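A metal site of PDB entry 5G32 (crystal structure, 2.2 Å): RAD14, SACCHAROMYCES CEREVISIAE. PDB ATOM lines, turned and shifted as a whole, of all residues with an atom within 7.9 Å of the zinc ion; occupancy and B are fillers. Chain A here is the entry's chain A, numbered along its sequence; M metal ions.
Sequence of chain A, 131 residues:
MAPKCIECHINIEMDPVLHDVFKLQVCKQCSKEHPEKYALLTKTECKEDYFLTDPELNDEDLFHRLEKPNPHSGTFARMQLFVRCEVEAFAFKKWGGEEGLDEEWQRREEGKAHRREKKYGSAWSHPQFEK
The side-chain sulfur of Cys 8 lies close to the backbone NH of Asn 11, at 3.4 Å. The backbone NH of Glu 7 sits close to the side-chain sulfur of Cys 5 (3.4 Å). N of Ile 10 lies close to SG of Cys 8 (3.6 Å). O of Asn 11 lies within hydrogen-bond range of N of Cys 5, at 2.9 Å. The side-chain amide nitrogen (ND2) of Asn 11 sits close to the side-chain sulfur (SG) of Cys 27 (3.3 Å).
Four residues have an atom within 4 Å of the zinc ion: Cys 5, Cys 8, Cys 27 and Cys 30. The nearest printed residue that does not touch the zinc ion is Glu 7 (4.3 Å).
The zinc ion is bound by SG of Cys 5 (2.2 Å), SG of Cys 30 (2.2 Å), SG of Cys 27 (2.4 Å) and SG of Cys 8 (2.5 Å). The zinc ion has four donor atoms within binding distance.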
ATOM      1  N   LYS A   4      12.822 -14.044  21.735  1.00  0.00           N
ATOM      2  CA  LYS A   4      14.229 -13.843  21.406  1.00  0.00           C
ATOM      3  C   LYS A   4      14.564 -12.370  21.037  1.00  0.00           C
ATOM      4  O   LYS A   4      13.770 -11.695  20.396  1.00  0.00           O
ATOM      5  CB  LYS A   4      14.619 -14.711  20.197  1.00  0.00           C
ATOM      6  CG  LYS A   4      14.243 -16.197  20.298  1.00  0.00           C
ATOM      7  CD  LYS A   4      15.175 -16.956  21.232  1.00  0.00           C
ATOM      8  CE  LYS A   4      14.600 -18.314  21.666  1.00  0.00           C
ATOM      9  NZ  LYS A   4      15.077 -19.461  20.876  1.00  0.00           N
ATOM     10  N   CYS A   5      15.764 -11.935  21.420  1.00  0.00           N
ATOM     11  CA  CYS A   5      16.374 -10.742  20.930  1.00  0.00           C
ATOM     12  C   CYS A   5      16.222 -10.599  19.422  1.00  0.00           C
ATOM     13  O   CYS A   5      16.563 -11.510  18.683  1.00  0.00           O
ATOM     14  CB  CYS A   5      17.846 -10.766  21.315  1.00  0.00           C
ATOM     15  SG  CYS A   5      18.880  -9.457  20.680  1.00  0.00           S
ATOM     16  N   ILE A   6      15.636  -9.489  18.954  1.00  0.00           N
ATOM     17  CA  ILE A   6      15.442  -9.257  17.527  1.00  0.00           C
ATOM     18  C   ILE A   6      16.745  -9.034  16.784  1.00  0.00           C
ATOM     19  O   ILE A   6      16.727  -8.982  15.615  1.00  0.00           O
ATOM     20  CB  ILE A   6      14.565  -8.015  17.220  1.00  0.00           C
ATOM     21  CG1 ILE A   6      15.300  -6.733  17.678  1.00  0.00           C
ATOM     22  CG2 ILE A   6      13.179  -8.127  17.811  1.00  0.00           C
ATOM     23  CD1 ILE A   6      14.451  -5.507  17.915  1.00  0.00           C
ATOM     24  N   GLU A   7      17.853  -8.797  17.455  1.00  0.00           N
ATOM     25  CA  GLU A   7      19.103  -8.550  16.726  1.00  0.00           C
ATOM     26  C   GLU A   7      19.800  -9.885  16.460  1.00  0.00           C
ATOM     27  O   GLU A   7      20.071 -10.216  15.342  1.00  0.00           O
ATOM     28  CB  GLU A   7      19.946  -7.586  17.572  1.00  0.00           C
ATOM     29  CG  GLU A   7      20.840  -6.584  16.883  1.00  0.00           C
ATOM     30  CD  GLU A   7      20.171  -5.709  15.812  1.00  0.00           C
ATOM     31  OE1 GLU A   7      19.187  -4.984  16.085  1.00  0.00           O
ATOM     32  OE2 GLU A   7      20.667  -5.746  14.685  1.00  0.00           O
ATOM     33  N   CYS A   8      20.020 -10.695  17.496  1.00  0.00           N
ATOM     34  CA  CYS A   8      20.759 -11.920  17.356  1.00  0.00           C
ATOM     35  C   CYS A   8      19.920 -13.204  17.126  1.00  0.00           C
ATOM     36  O   CYS A   8      20.446 -14.205  16.642  1.00  0.00           O
ATOM     37  CB  CYS A   8      21.700 -12.104  18.550  1.00  0.00           C
ATOM     38  SG  CYS A   8      20.926 -12.466  20.140  1.00  0.00           S
ATOM     39  N   HIS A   9      18.639 -13.160  17.494  1.00  0.00           N
ATOM     40  CA  HIS A   9      17.702 -14.293  17.445  1.00  0.00           C
ATOM     41  C   HIS A   9      18.012 -15.495  18.386  1.00  0.00           C
ATOM     42  O   HIS A   9      17.440 -16.580  18.220  1.00  0.00           O
ATOM     43  CB  HIS A   9      17.469 -14.735  15.992  1.00  0.00           C
ATOM     44  CG  HIS A   9      17.258 -13.575  15.065  1.00  0.00           C
ATOM     45  ND1 HIS A   9      16.103 -12.812  15.057  1.00  0.00           N
ATOM     46  CD2 HIS A   9      18.078 -13.024  14.128  1.00  0.00           C
ATOM     47  CE1 HIS A   9      16.205 -11.856  14.149  1.00  0.00           C
ATOM     48  NE2 HIS A   9      17.386 -11.971  13.559  1.00  0.00           N
ATOM     49  N   ILE A  10      18.805 -15.229  19.422  1.00  0.00           N
ATOM     50  CA  ILE A  10      19.385 -16.227  20.295  1.00  0.00           C
ATOM     51  C   ILE A  10      19.151 -15.935  21.758  1.00  0.00           C
ATOM     52  O   ILE A  10      18.591 -16.776  22.448  1.00  0.00           O
ATOM     53  CB  ILE A  10      20.899 -16.307  20.050  1.00  0.00           C
ATOM     54  CG1 ILE A  10      21.107 -16.855  18.605  1.00  0.00           C
ATOM     55  CG2 ILE A  10      21.572 -17.237  21.095  1.00  0.00           C
ATOM     56  CD1 ILE A  10      22.521 -16.855  18.128  1.00  0.00           C
ATOM     57  N   ASN A  11      19.630 -14.764  22.256  1.00  0.00           N
ATOM     58  CA  ASN A  11      19.471 -14.380  23.679  1.00  0.00           C
ATOM     59  C   ASN A  11      17.988 -14.203  24.032  1.00  0.00           C
ATOM     60  O   ASN A  11      17.200 -13.696  23.265  1.00  0.00           O
ATOM     61  CB  ASN A  11      20.322 -13.167  24.104  1.00  0.00           C
ATOM     62  CG  ASN A  11      21.732 -13.550  24.604  1.00  0.00           C
ATOM     63  OD1 ASN A  11      21.933 -14.610  25.222  1.00  0.00           O
ATOM     64  ND2 ASN A  11      22.707 -12.680  24.348  1.00  0.00           N
ATOM     65  N   ILE A  12      17.637 -14.713  25.192  1.00  0.00           N
ATOM     66  CA  ILE A  12      16.314 -14.525  25.701  1.00  0.00           C
ATOM     67  C   ILE A  12      16.305 -13.499  26.863  1.00  0.00           C
ATOM     68  O   ILE A  12      15.232 -13.131  27.282  1.00  0.00           O
ATOM     69  CB  ILE A  12      15.649 -15.844  26.107  1.00  0.00           C
ATOM     70  CG1 ILE A  12      16.454 -16.590  27.174  1.00  0.00           C
ATOM     71  CG2 ILE A  12      15.471 -16.737  24.878  1.00  0.00           C
ATOM     72  CD1 ILE A  12      15.722 -17.804  27.724  1.00  0.00           C
ATOM     73  N   GLU A  13      17.459 -13.059  27.380  1.00  0.00           N
ATOM     74  CA  GLU A  13      17.503 -12.090  28.504  1.00  0.00           C
ATOM     75  C   GLU A  13      17.795 -10.741  27.904  1.00  0.00           C
ATOM     76  O   GLU A  13      18.840 -10.577  27.320  1.00  0.00           O
ATOM     77  CB  GLU A  13      18.587 -12.411  29.480  1.00  0.00           C
ATOM     78  CG  GLU A  13      18.450 -13.799  30.059  1.00  0.00           C
ATOM     79  CD  GLU A  13      17.595 -13.814  31.275  1.00  0.00           C
ATOM     80  OE1 GLU A  13      17.614 -12.785  32.006  1.00  0.00           O
ATOM     81  OE2 GLU A  13      16.933 -14.854  31.500  1.00  0.00           O
ATOM     82  N   MET A  14      16.860  -9.807  28.050  1.00  0.00           N
ATOM     83  CA  MET A  14      16.927  -8.541  27.343  1.00  0.00           C
ATOM     84  C   MET A  14      17.663  -7.534  28.190  1.00  0.00           C
ATOM     85  O   MET A  14      17.717  -7.658  29.413  1.00  0.00           O
ATOM     86  CB  MET A  14      15.520  -8.078  26.956  1.00  0.00           C
ATOM     87  CG  MET A  14      14.755  -9.051  26.075  1.00  0.00           C
ATOM     88  SD  MET A  14      15.636  -9.544  24.540  1.00  0.00           S
ATOM     89  CE  MET A  14      15.057 -11.249  24.414  1.00  0.00           C
ATOM     90  N   GLN A  25      13.191  -5.262  22.401  1.00  0.00           N
ATOM     91  CA  GLN A  25      13.571  -6.649  22.727  1.00  0.00           C
ATOM     92  C   GLN A  25      14.984  -6.884  22.241  1.00  0.00           C
ATOM     93  O   GLN A  25      15.191  -7.526  21.185  1.00  0.00           O
ATOM     94  CB  GLN A  25      12.660  -7.671  22.016  1.00  0.00           C
ATOM     95  CG  GLN A  25      11.194  -7.569  22.339  1.00  0.00           C
ATOM     96  CD  GLN A  25      10.865  -7.906  23.780  1.00  0.00           C
ATOM     97  OE1 GLN A  25      11.655  -8.535  24.514  1.00  0.00           O
ATOM     98  NE2 GLN A  25       9.649  -7.523  24.203  1.00  0.00           N
ATOM     99  N   VAL A  26      15.953  -6.353  23.003  1.00  0.00           N
ATOM    100  CA  VAL A  26      17.381  -6.361  22.628  1.00  0.00           C
ATOM    101  C   VAL A  26      18.257  -6.654  23.836  1.00  0.00           C
ATOM    102  O   VAL A  26      18.000  -6.145  24.924  1.00  0.00           O
ATOM    103  CB  VAL A  26      17.852  -5.056  22.034  1.00  0.00           C
ATOM    104  CG1 VAL A  26      19.042  -5.284  21.147  1.00  0.00           C
ATOM    105  CG2 VAL A  26      16.767  -4.449  21.188  1.00  0.00           C
ATOM    106  N   CYS A  27      19.244  -7.505  23.625  1.00  0.00           N
ATOM    107  CA  CYS A  27      20.052  -8.049  24.680  1.00  0.00           C
ATOM    108  C   CYS A  27      21.212  -7.088  24.873  1.00  0.00           C
ATOM    109  O   CYS A  27      21.454  -6.329  23.999  1.00  0.00           O
ATOM    110  CB  CYS A  27      20.469  -9.509  24.401  1.00  0.00           C
ATOM    111  SG  CYS A  27      21.749  -9.747  23.160  1.00  0.00           S
ATOM    112  N   LYS A  28      21.864  -7.113  26.026  1.00  0.00           N
ATOM    113  CA  LYS A  28      22.910  -6.173  26.349  1.00  0.00           C
ATOM    114  C   LYS A  28      24.019  -6.276  25.343  1.00  0.00           C
ATOM    115  O   LYS A  28      24.570  -5.259  24.931  1.00  0.00           O
ATOM    116  CB  LYS A  28      23.452  -6.371  27.751  1.00  0.00           C
ATOM    117  CG  LYS A  28      24.363  -5.212  28.188  1.00  0.00           C
ATOM    118  CD  LYS A  28      24.075  -4.693  29.618  1.00  0.00           C
ATOM    119  CE  LYS A  28      24.846  -3.397  29.968  1.00  0.00           C
ATOM    120  NZ  LYS A  28      24.015  -2.298  30.556  1.00  0.00           N
ATOM    121  N   GLN A  29      24.334  -7.489  24.908  1.00  0.00           N
ATOM    122  CA  GLN A  29      25.470  -7.699  24.008  1.00  0.00           C
ATOM    123  C   GLN A  29      25.217  -7.126  22.625  1.00  0.00           C
ATOM    124  O   GLN A  29      26.077  -6.430  22.082  1.00  0.00           O
ATOM    125  CB  GLN A  29      25.916  -9.188  23.936  1.00  0.00           C
ATOM    126  CG  GLN A  29      26.847  -9.558  22.776  1.00  0.00           C
ATOM    127  CD  GLN A  29      27.406 -10.939  22.910  1.00  0.00           C
ATOM    128  OE1 GLN A  29      26.846 -11.800  23.574  1.00  0.00           O
ATOM    129  NE2 GLN A  29      28.518 -11.153  22.317  1.00  0.00           N
ATOM    130  N   CYS A  30      24.026  -7.380  22.081  1.00  0.00           N
ATOM    131  CA  CYS A  30      23.684  -6.817  20.796  1.00  0.00           C
ATOM    132  C   CYS A  30      23.625  -5.265  20.855  1.00  0.00           C
ATOM    133  O   CYS A  30      24.030  -4.594  19.889  1.00  0.00           O
ATOM    134  CB  CYS A  30      22.394  -7.397  20.263  1.00  0.00           C
ATOM    135  SG  CYS A  30      22.555  -9.107  19.712  1.00  0.00           S
ATOM    136  N   SER A  31      23.127  -4.689  21.952  1.00  0.00           N
ATOM    137  CA  SER A  31      23.166  -3.211  22.075  1.00  0.00           C
ATOM    138  C   SER A  31      24.594  -2.671  21.943  1.00  0.00           C
ATOM    139  O   SER A  31      24.792  -1.746  21.213  1.00  0.00           O
ATOM    140  CB  SER A  31      22.524  -2.689  23.349  1.00  0.00           C
ATOM    141  OG  SER A  31      23.310  -3.007  24.462  1.00  0.00           O
ATOM    142  N   GLU A  33      27.071  -4.158  20.377  1.00  0.00           N
ATOM    143  CA  GLU A  33      27.546  -4.471  19.033  1.00  0.00           C
ATOM    144  C   GLU A  33      26.888  -3.528  17.969  1.00  0.00           C
ATOM    145  O   GLU A  33      27.406  -3.409  16.843  1.00  0.00           O
ATOM    146  CB  GLU A  33      27.322  -5.961  18.720  1.00  0.00           C
ATOM    147  CG  GLU A  33      28.141  -6.860  19.659  1.00  0.00           C
ATOM    148  CD  GLU A  33      27.871  -8.392  19.584  1.00  0.00           C
ATOM    149  OE1 GLU A  33      26.775  -8.834  19.127  1.00  0.00           O
ATOM    150  OE2 GLU A  33      28.770  -9.181  20.043  1.00  0.00           O
ATOM    151  N   HIS A  34      25.780  -2.848  18.335  1.00  0.00           N
ATOM    152  CA  HIS A  34      25.100  -2.018  17.383  1.00  0.00           C
ATOM    153  C   HIS A  34      24.799  -0.650  17.930  1.00  0.00           C
ATOM    154  O   HIS A  34      23.636  -0.302  18.087  1.00  0.00           O
ATOM    155  CB  HIS A  34      23.829  -2.702  16.898  1.00  0.00           C
ATOM    156  CG  HIS A  34      24.111  -3.879  16.067  1.00  0.00           C
ATOM    157  ND1 HIS A  34      24.752  -3.771  14.860  1.00  0.00           N
ATOM    158  CD2 HIS A  34      23.976  -5.207  16.308  1.00  0.00           C
ATOM    159  CE1 HIS A  34      24.981  -4.984  14.382  1.00  0.00           C
ATOM    160  NE2 HIS A  34      24.497  -5.862  15.239  1.00  0.00           N
ATOM    161  N   TYR A  38      21.464   1.562  19.134  1.00  0.00           N
ATOM    162  CA  TYR A  38      21.094   1.360  20.551  1.00  0.00           C
ATOM    163  C   TYR A  38      21.836   2.209  21.524  1.00  0.00           C
ATOM    164  O   TYR A  38      21.585   2.109  22.693  1.00  0.00           O
ATOM    165  CB  TYR A  38      21.248  -0.110  20.930  1.00  0.00           C
ATOM    166  CG  TYR A  38      20.404  -1.012  20.065  1.00  0.00           C
ATOM    167  CD1 TYR A  38      19.025  -0.890  20.042  1.00  0.00           C
ATOM    168  CD2 TYR A  38      20.969  -1.980  19.266  1.00  0.00           C
ATOM    169  CE1 TYR A  38      18.237  -1.694  19.231  1.00  0.00           C
ATOM    170  CE2 TYR A  38      20.174  -2.824  18.442  1.00  0.00           C
ATOM    171  CZ  TYR A  38      18.813  -2.667  18.439  1.00  0.00           C
ATOM    172  OH  TYR A  38      18.008  -3.457  17.677  1.00  0.00           O
HETATM  173 ZN    ZN M   1      20.954 -10.133  20.909  1.00  0.00          ZN
